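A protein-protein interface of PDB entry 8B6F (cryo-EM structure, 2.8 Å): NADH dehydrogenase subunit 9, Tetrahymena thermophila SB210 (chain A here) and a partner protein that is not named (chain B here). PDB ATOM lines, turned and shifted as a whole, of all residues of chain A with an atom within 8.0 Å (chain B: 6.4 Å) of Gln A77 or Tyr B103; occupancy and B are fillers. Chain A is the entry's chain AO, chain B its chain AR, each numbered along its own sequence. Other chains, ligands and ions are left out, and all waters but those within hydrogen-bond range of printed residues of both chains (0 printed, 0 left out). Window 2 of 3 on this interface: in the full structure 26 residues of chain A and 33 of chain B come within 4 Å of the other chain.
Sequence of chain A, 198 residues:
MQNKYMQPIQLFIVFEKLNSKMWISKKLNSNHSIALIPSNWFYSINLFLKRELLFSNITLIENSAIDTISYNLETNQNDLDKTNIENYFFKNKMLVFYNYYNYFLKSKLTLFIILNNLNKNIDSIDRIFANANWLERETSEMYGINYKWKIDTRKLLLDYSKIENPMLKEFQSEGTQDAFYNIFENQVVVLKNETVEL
The side-chain amide oxygen (OD1) of Asn A72 sits close to the backbone NH (N) of Cys B137, 3.2 Å away. NZ of Lys B104 lies within salt-bridge range of OE1 of Glu A74, 2.9 Å away.
The backbone carbonyl oxygen (O) of Leu A73 lies within hydrogen-bond range of the side-chain amide nitrogen (NE2) of Gln A77, at 2.8 Å. The backbone carbonyl oxygen (O) of Glu A74 is in hydrogen-bond range of the side-chain amide nitrogen (NE2) of Gln A77 (2.8 Å). NE2 of Gln A77 sits close to N of Thr A75, 3.5 Å away. SD of Met B1 sits at hydrogen-bond distance from N of Lys B104, 3.6 Å away. The backbone NH (N) of Trp B105 is in hydrogen-bond range of the backbone carbonyl oxygen (O) of Phe B136, at 2.9 Å.
Asn A72 touches Lys B104. OD1 of Asn A72 touches C of Phe B136, 3.7 Å away. CD of Pro B100 touches O of Glu A74 (3.5 Å). Gln A77 touches Tyr B103.
Printed residues of chain B within 4 Å of Glu A74: Pro B100 and Lys B104. Gln A77 touches just one residue of chain B: Tyr B103 (3.6 Å). Printed residues of chain A within 4 Å of Pro B100: Glu A74 (3.5 Å). No residue of chain A comes within 4 Å of Gly B102. Tyr B103 touches just one residue of chain A: Gln A77 (3.6 Å). Of the printed residues of chain A, Phe B136 touches Asn A72. Of the printed residues of chain A, Cys B137 touches Asn A72. The nearest residue of chain B that does not touch Gln A77 is Pro B100 (4.1 Å). The nearest printed residue of chain A that does not touch Pro B100 is Thr A75 (4.1 Å).
Of the 12 printed residues of chain A, 3 touch a printed residue of chain B. Printed residues of chain B that touch a printed residue of chain A: Pro B100, Tyr B103, Lys B104, Phe B136 and Cys B137. Hydrophobic or aromatic side chains of chain B that line the printed part of chain A: Pro B100 and Tyr B103. Among the printed residues, 6 pairs touch across the chains. Among the printed residues, Asp or Glu carboxylates within 4 Å of a Lys or Arg side-chain nitrogen of the other chain: Glu A74 with Lys B104.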
ATOM      1  N   TYR A  71      33.305  -7.699 -18.026  1.00  0.00           N
ATOM      2  CA  TYR A  71      33.683  -8.648 -19.063  1.00  0.00           C
ATOM      3  C   TYR A  71      32.734  -9.839 -19.053  1.00  0.00           C
ATOM      4  O   TYR A  71      32.511 -10.458 -18.009  1.00  0.00           O
ATOM      5  CB  TYR A  71      35.120  -9.121 -18.852  1.00  0.00           C
ATOM      6  CG  TYR A  71      35.629 -10.029 -19.946  1.00  0.00           C
ATOM      7  CD1 TYR A  71      36.221  -9.507 -21.090  1.00  0.00           C
ATOM      8  CD2 TYR A  71      35.520 -11.408 -19.836  1.00  0.00           C
ATOM      9  CE1 TYR A  71      36.687 -10.333 -22.092  1.00  0.00           C
ATOM     10  CE2 TYR A  71      35.984 -12.242 -20.833  1.00  0.00           C
ATOM     11  CZ  TYR A  71      36.567 -11.698 -21.958  1.00  0.00           C
ATOM     12  OH  TYR A  71      37.030 -12.524 -22.954  1.00  0.00           O
ATOM     13  N   ASN A  72      32.184 -10.160 -20.222  1.00  0.00           N
ATOM     14  CA  ASN A  72      31.267 -11.281 -20.374  1.00  0.00           C
ATOM     15  C   ASN A  72      31.547 -11.982 -21.692  1.00  0.00           C
ATOM     16  O   ASN A  72      31.819 -11.330 -22.704  1.00  0.00           O
ATOM     17  CB  ASN A  72      29.806 -10.821 -20.341  1.00  0.00           C
ATOM     18  CG  ASN A  72      29.468 -10.050 -19.087  1.00  0.00           C
ATOM     19  OD1 ASN A  72      29.868 -10.423 -17.987  1.00  0.00           O
ATOM     20  ND2 ASN A  72      28.733  -8.957 -19.247  1.00  0.00           N
ATOM     21  N   LEU A  73      31.470 -13.311 -21.680  1.00  0.00           N
ATOM     22  CA  LEU A  73      31.625 -14.099 -22.898  1.00  0.00           C
ATOM     23  C   LEU A  73      30.335 -14.002 -23.700  1.00  0.00           C
ATOM     24  O   LEU A  73      29.300 -14.541 -23.295  1.00  0.00           O
ATOM     25  CB  LEU A  73      31.956 -15.550 -22.564  1.00  0.00           C
ATOM     26  CG  LEU A  73      33.324 -15.799 -21.928  1.00  0.00           C
ATOM     27  CD1 LEU A  73      33.472 -17.259 -21.559  1.00  0.00           C
ATOM     28  CD2 LEU A  73      34.446 -15.373 -22.860  1.00  0.00           C
ATOM     29  N   GLU A  74      30.395 -13.314 -24.840  1.00  0.00           N
ATOM     30  CA  GLU A  74      29.191 -13.073 -25.622  1.00  0.00           C
ATOM     31  C   GLU A  74      28.838 -14.251 -26.521  1.00  0.00           C
ATOM     32  O   GLU A  74      27.666 -14.425 -26.869  1.00  0.00           O
ATOM     33  CB  GLU A  74      29.367 -11.805 -26.458  1.00  0.00           C
ATOM     34  CG  GLU A  74      29.603 -10.554 -25.621  1.00  0.00           C
ATOM     35  CD  GLU A  74      28.391 -10.160 -24.803  1.00  0.00           C
ATOM     36  OE1 GLU A  74      27.322 -10.780 -24.982  1.00  0.00           O
ATOM     37  OE2 GLU A  74      28.505  -9.227 -23.981  1.00  0.00           O
ATOM     38  N   THR A  75      29.820 -15.067 -26.899  1.00  0.00           N
ATOM     39  CA  THR A  75      29.576 -16.232 -27.734  1.00  0.00           C
ATOM     40  C   THR A  75      30.418 -17.394 -27.231  1.00  0.00           C
ATOM     41  O   THR A  75      31.463 -17.198 -26.606  1.00  0.00           O
ATOM     42  CB  THR A  75      29.895 -15.959 -29.210  1.00  0.00           C
ATOM     43  OG1 THR A  75      31.292 -15.680 -29.358  1.00  0.00           O
ATOM     44  CG2 THR A  75      29.083 -14.779 -29.723  1.00  0.00           C
ATOM     45  N   ASN A  76      29.954 -18.609 -27.517  1.00  0.00           N
ATOM     46  CA  ASN A  76      30.650 -19.829 -27.118  1.00  0.00           C
ATOM     47  C   ASN A  76      30.938 -19.826 -25.620  1.00  0.00           C
ATOM     48  O   ASN A  76      32.064 -20.056 -25.174  1.00  0.00           O
ATOM     49  CB  ASN A  76      31.938 -20.005 -27.920  1.00  0.00           C
ATOM     50  CG  ASN A  76      31.682 -20.189 -29.400  1.00  0.00           C
ATOM     51  OD1 ASN A  76      30.661 -20.746 -29.798  1.00  0.00           O
ATOM     52  ND2 ASN A  76      32.609 -19.718 -30.224  1.00  0.00           N
ATOM     53  N   GLN A  77      29.896 -19.552 -24.833  1.00  0.00           N
ATOM     54  CA  GLN A  77      30.065 -19.484 -23.386  1.00  0.00           C
ATOM     55  C   GLN A  77      30.458 -20.838 -22.811  1.00  0.00           C
ATOM     56  O   GLN A  77      31.299 -20.918 -21.909  1.00  0.00           O
ATOM     57  CB  GLN A  77      28.782 -18.977 -22.725  1.00  0.00           C
ATOM     58  CG  GLN A  77      28.462 -17.519 -23.008  1.00  0.00           C
ATOM     59  CD  GLN A  77      27.881 -17.298 -24.389  1.00  0.00           C
ATOM     60  OE1 GLN A  77      27.882 -18.199 -25.227  1.00  0.00           O
ATOM     61  NE2 GLN A  77      27.371 -16.097 -24.631  1.00  0.00           N
ATOM     62  N   ASN A  78      29.861 -21.916 -23.321  1.00  0.00           N
ATOM     63  CA  ASN A  78      30.120 -23.241 -22.770  1.00  0.00           C
ATOM     64  C   ASN A  78      31.522 -23.744 -23.087  1.00  0.00           C
ATOM     65  O   ASN A  78      32.034 -24.601 -22.359  1.00  0.00           O
ATOM     66  CB  ASN A  78      29.083 -24.234 -23.298  1.00  0.00           C
ATOM     67  CG  ASN A  78      29.272 -25.625 -22.732  1.00  0.00           C
ATOM     68  OD1 ASN A  78      29.903 -26.480 -23.352  1.00  0.00           O
ATOM     69  ND2 ASN A  78      28.726 -25.859 -21.545  1.00  0.00           N
ATOM     70  N   ASP A  79      32.152 -23.238 -24.147  1.00  0.00           N
ATOM     71  CA  ASP A  79      33.475 -23.712 -24.533  1.00  0.00           C
ATOM     72  C   ASP A  79      34.571 -23.270 -23.574  1.00  0.00           C
ATOM     73  O   ASP A  79      35.684 -23.800 -23.651  1.00  0.00           O
ATOM     74  CB  ASP A  79      33.813 -23.228 -25.944  1.00  0.00           C
ATOM     75  CG  ASP A  79      32.859 -23.771 -26.988  1.00  0.00           C
ATOM     76  OD1 ASP A  79      32.215 -24.806 -26.721  1.00  0.00           O
ATOM     77  OD2 ASP A  79      32.757 -23.166 -28.075  1.00  0.00           O
ATOM     78  N   LEU A  80      34.292 -22.323 -22.681  1.00  0.00           N
ATOM     79  CA  LEU A  80      35.307 -21.863 -21.745  1.00  0.00           C
ATOM     80  C   LEU A  80      35.805 -23.019 -20.889  1.00  0.00           C
ATOM     81  O   LEU A  80      35.023 -23.848 -20.417  1.00  0.00           O
ATOM     82  CB  LEU A  80      34.741 -20.756 -20.854  1.00  0.00           C
ATOM     83  CG  LEU A  80      35.739 -20.092 -19.899  1.00  0.00           C
ATOM     84  CD1 LEU A  80      36.752 -19.261 -20.672  1.00  0.00           C
ATOM     85  CD2 LEU A  80      35.022 -19.245 -18.862  1.00  0.00           C
ATOM     86  N   ASP A  81      37.119 -23.069 -20.690  1.00  0.00           N
ATOM     87  CA  ASP A  81      37.760 -24.084 -19.869  1.00  0.00           C
ATOM     88  C   ASP A  81      38.473 -23.418 -18.702  1.00  0.00           C
ATOM     89  O   ASP A  81      38.862 -22.249 -18.775  1.00  0.00           O
ATOM     90  CB  ASP A  81      38.751 -24.919 -20.687  1.00  0.00           C
ATOM     91  CG  ASP A  81      39.737 -24.063 -21.452  1.00  0.00           C
ATOM     92  OD1 ASP A  81      39.668 -22.824 -21.325  1.00  0.00           O
ATOM     93  OD2 ASP A  81      40.577 -24.627 -22.184  1.00  0.00           O
ATOM     94  N   PHE A  90      36.448 -12.363 -14.568  1.00  0.00           N
ATOM     95  CA  PHE A  90      35.151 -12.254 -13.914  1.00  0.00           C
ATOM     96  C   PHE A  90      35.308 -11.845 -12.454  1.00  0.00           C
ATOM     97  O   PHE A  90      36.135 -12.400 -11.724  1.00  0.00           O
ATOM     98  CB  PHE A  90      34.402 -13.582 -14.010  1.00  0.00           C
ATOM     99  CG  PHE A  90      34.257 -14.096 -15.413  1.00  0.00           C
ATOM    100  CD1 PHE A  90      33.339 -13.531 -16.281  1.00  0.00           C
ATOM    101  CD2 PHE A  90      35.030 -15.153 -15.861  1.00  0.00           C
ATOM    102  CE1 PHE A  90      33.199 -14.004 -17.570  1.00  0.00           C
ATOM    103  CE2 PHE A  90      34.895 -15.632 -17.150  1.00  0.00           C
ATOM    104  CZ  PHE A  90      33.978 -15.056 -18.005  1.00  0.00           C
ATOM    105  N   MET B   1      27.692 -17.060 -14.823  1.00  0.00           N
ATOM    106  CA  MET B   1      26.619 -16.191 -14.265  1.00  0.00           C
ATOM    107  C   MET B   1      26.050 -16.790 -12.980  1.00  0.00           C
ATOM    108  O   MET B   1      25.190 -16.193 -12.337  1.00  0.00           O
ATOM    109  CB  MET B   1      25.508 -15.988 -15.297  1.00  0.00           C
ATOM    110  CG  MET B   1      24.453 -14.980 -14.881  1.00  0.00           C
ATOM    111  SD  MET B   1      23.463 -14.403 -16.269  1.00  0.00           S
ATOM    112  CE  MET B   1      22.692 -15.926 -16.799  1.00  0.00           C
ATOM    113  N   ILE B  87      17.676  -9.330 -16.667  1.00  0.00           N
ATOM    114  CA  ILE B  87      18.309 -10.122 -17.715  1.00  0.00           C
ATOM    115  C   ILE B  87      17.558  -9.883 -19.018  1.00  0.00           C
ATOM    116  O   ILE B  87      16.347 -10.107 -19.097  1.00  0.00           O
ATOM    117  CB  ILE B  87      18.341 -11.616 -17.353  1.00  0.00           C
ATOM    118  CG1 ILE B  87      19.383 -11.859 -16.258  1.00  0.00           C
ATOM    119  CG2 ILE B  87      18.627 -12.473 -18.589  1.00  0.00           C
ATOM    120  CD1 ILE B  87      19.497 -13.294 -15.811  1.00  0.00           C
ATOM    121  N   GLN B  88      18.279  -9.423 -20.037  1.00  0.00           N
ATOM    122  CA  GLN B  88      17.708  -9.179 -21.356  1.00  0.00           C
ATOM    123  C   GLN B  88      17.834 -10.459 -22.175  1.00  0.00           C
ATOM    124  O   GLN B  88      18.943 -10.881 -22.514  1.00  0.00           O
ATOM    125  CB  GLN B  88      18.419  -8.014 -22.039  1.00  0.00           C
ATOM    126  CG  GLN B  88      17.873  -7.653 -23.411  1.00  0.00           C
ATOM    127  CD  GLN B  88      16.489  -7.040 -23.350  1.00  0.00           C
ATOM    128  OE1 GLN B  88      15.947  -6.810 -22.272  1.00  0.00           O
ATOM    129  NE2 GLN B  88      15.912  -6.767 -24.515  1.00  0.00           N
ATOM    130  N   ASP B  89      16.700 -11.073 -22.490  1.00  0.00           N
ATOM    131  CA  ASP B  89      16.667 -12.305 -23.258  1.00  0.00           C
ATOM    132  C   ASP B  89      16.558 -12.003 -24.748  1.00  0.00           C
ATOM    133  O   ASP B  89      16.272 -10.879 -25.166  1.00  0.00           O
ATOM    134  CB  ASP B  89      15.495 -13.180 -22.811  1.00  0.00           C
ATOM    135  CG  ASP B  89      15.608 -13.610 -21.363  1.00  0.00           C
ATOM    136  OD1 ASP B  89      16.738 -13.877 -20.907  1.00  0.00           O
ATOM    137  OD2 ASP B  89      14.564 -13.678 -20.678  1.00  0.00           O
ATOM    138  N   PRO B 100      24.174 -14.658 -28.960  1.00  0.00           N
ATOM    139  CA  PRO B 100      23.058 -14.913 -28.043  1.00  0.00           C
ATOM    140  C   PRO B 100      23.074 -13.976 -26.847  1.00  0.00           C
ATOM    141  O   PRO B 100      24.121 -13.477 -26.427  1.00  0.00           O
ATOM    142  CB  PRO B 100      23.277 -16.368 -27.613  1.00  0.00           C
ATOM    143  CG  PRO B 100      24.733 -16.591 -27.781  1.00  0.00           C
ATOM    144  CD  PRO B 100      25.143 -15.768 -28.966  1.00  0.00           C
ATOM    145  N   GLU B 101      21.886 -13.740 -26.299  1.00  0.00           N
ATOM    146  CA  GLU B 101      21.696 -12.883 -25.140  1.00  0.00           C
ATOM    147  C   GLU B 101      21.159 -13.704 -23.973  1.00  0.00           C
ATOM    148  O   GLU B 101      20.831 -14.885 -24.107  1.00  0.00           O
ATOM    149  CB  GLU B 101      20.739 -11.729 -25.458  1.00  0.00           C
ATOM    150  CG  GLU B 101      21.198 -10.850 -26.606  1.00  0.00           C
ATOM    151  CD  GLU B 101      20.265  -9.684 -26.853  1.00  0.00           C
ATOM    152  OE1 GLU B 101      19.364  -9.458 -26.019  1.00  0.00           O
ATOM    153  OE2 GLU B 101      20.430  -8.995 -27.880  1.00  0.00           O
ATOM    154  N   GLY B 102      21.069 -13.055 -22.815  1.00  0.00           N
ATOM    155  CA  GLY B 102      20.577 -13.695 -21.614  1.00  0.00           C
ATOM    156  C   GLY B 102      21.638 -14.301 -20.726  1.00  0.00           C
ATOM    157  O   GLY B 102      21.290 -14.976 -19.751  1.00  0.00           O
ATOM    158  N   TYR B 103      22.917 -14.088 -21.029  1.00  0.00           N
ATOM    159  CA  TYR B 103      24.018 -14.619 -20.238  1.00  0.00           C
ATOM    160  C   TYR B 103      24.628 -13.575 -19.315  1.00  0.00           C
ATOM    161  O   TYR B 103      25.686 -13.823 -18.729  1.00  0.00           O
ATOM    162  CB  TYR B 103      25.102 -15.183 -21.159  1.00  0.00           C
ATOM    163  CG  TYR B 103      24.644 -16.326 -22.035  1.00  0.00           C
ATOM    164  CD1 TYR B 103      23.839 -16.096 -23.142  1.00  0.00           C
ATOM    165  CD2 TYR B 103      25.031 -17.631 -21.768  1.00  0.00           C
ATOM    166  CE1 TYR B 103      23.423 -17.129 -23.948  1.00  0.00           C
ATOM    167  CE2 TYR B 103      24.619 -18.675 -22.572  1.00  0.00           C
ATOM    168  CZ  TYR B 103      23.816 -18.414 -23.662  1.00  0.00           C
ATOM    169  OH  TYR B 103      23.397 -19.441 -24.473  1.00  0.00           O
ATOM    170  N   LYS B 104      23.992 -12.416 -19.174  1.00  0.00           N
ATOM    171  CA  LYS B 104      24.554 -11.330 -18.386  1.00  0.00           C
ATOM    172  C   LYS B 104      23.425 -10.430 -17.910  1.00  0.00           C
ATOM    173  O   LYS B 104      22.400 -10.290 -18.581  1.00  0.00           O
ATOM    174  CB  LYS B 104      25.574 -10.526 -19.198  1.00  0.00           C
ATOM    175  CG  LYS B 104      25.034  -9.991 -20.517  1.00  0.00           C
ATOM    176  CD  LYS B 104      26.140  -9.407 -21.377  1.00  0.00           C
ATOM    177  CE  LYS B 104      25.594  -8.844 -22.677  1.00  0.00           C
ATOM    178  NZ  LYS B 104      25.011  -9.903 -23.543  1.00  0.00           N
ATOM    179  N   TRP B 105      23.630  -9.822 -16.745  1.00  0.00           N
ATOM    180  CA  TRP B 105      22.662  -8.890 -16.187  1.00  0.00           C
ATOM    181  C   TRP B 105      22.875  -7.513 -16.798  1.00  0.00           C
ATOM    182  O   TRP B 105      23.989  -6.981 -16.780  1.00  0.00           O
ATOM    183  CB  TRP B 105      22.792  -8.817 -14.666  1.00  0.00           C
ATOM    184  CG  TRP B 105      22.411 -10.077 -13.966  1.00  0.00           C
ATOM    185  CD1 TRP B 105      23.186 -11.184 -13.794  1.00  0.00           C
ATOM    186  CD2 TRP B 105      21.156 -10.364 -13.339  1.00  0.00           C
ATOM    187  NE1 TRP B 105      22.493 -12.144 -13.099  1.00  0.00           N
ATOM    188  CE2 TRP B 105      21.242 -11.665 -12.810  1.00  0.00           C
ATOM    189  CE3 TRP B 105      19.967  -9.646 -13.177  1.00  0.00           C
ATOM    190  CZ2 TRP B 105      20.186 -12.263 -12.125  1.00  0.00           C
ATOM    191  CZ3 TRP B 105      18.919 -10.241 -12.499  1.00  0.00           C
ATOM    192  CH2 TRP B 105      19.034 -11.539 -11.982  1.00  0.00           C
ATOM    193  N   PHE B 136      26.901  -6.800 -16.633  1.00  0.00           N
ATOM    194  CA  PHE B 136      27.654  -7.425 -15.559  1.00  0.00           C
ATOM    195  C   PHE B 136      27.457  -8.931 -15.623  1.00  0.00           C
ATOM    196  O   PHE B 136      26.405  -9.417 -16.046  1.00  0.00           O
ATOM    197  CB  PHE B 136      27.224  -6.882 -14.192  1.00  0.00           C
ATOM    198  CG  PHE B 136      27.432  -5.403 -14.043  1.00  0.00           C
ATOM    199  CD1 PHE B 136      28.634  -4.900 -13.577  1.00  0.00           C
ATOM    200  CD2 PHE B 136      26.426  -4.514 -14.383  1.00  0.00           C
ATOM    201  CE1 PHE B 136      28.828  -3.540 -13.446  1.00  0.00           C
ATOM    202  CE2 PHE B 136      26.612  -3.154 -14.254  1.00  0.00           C
ATOM    203  CZ  PHE B 136      27.815  -2.666 -13.786  1.00  0.00           C
ATOM    204  N   CYS B 137      28.480  -9.669 -15.189  1.00  0.00           N
ATOM    205  CA  CYS B 137      28.403 -11.125 -15.215  1.00  0.00           C
ATOM    206  C   CYS B 137      27.443 -11.658 -14.160  1.00  0.00           C
ATOM    207  O   CYS B 137      26.763 -12.662 -14.397  1.00  0.00           O
ATOM    208  CB  CYS B 137      29.793 -11.731 -15.023  1.00  0.00           C
ATOM    209  SG  CYS B 137      30.626 -11.247 -13.498  1.00  0.00           S
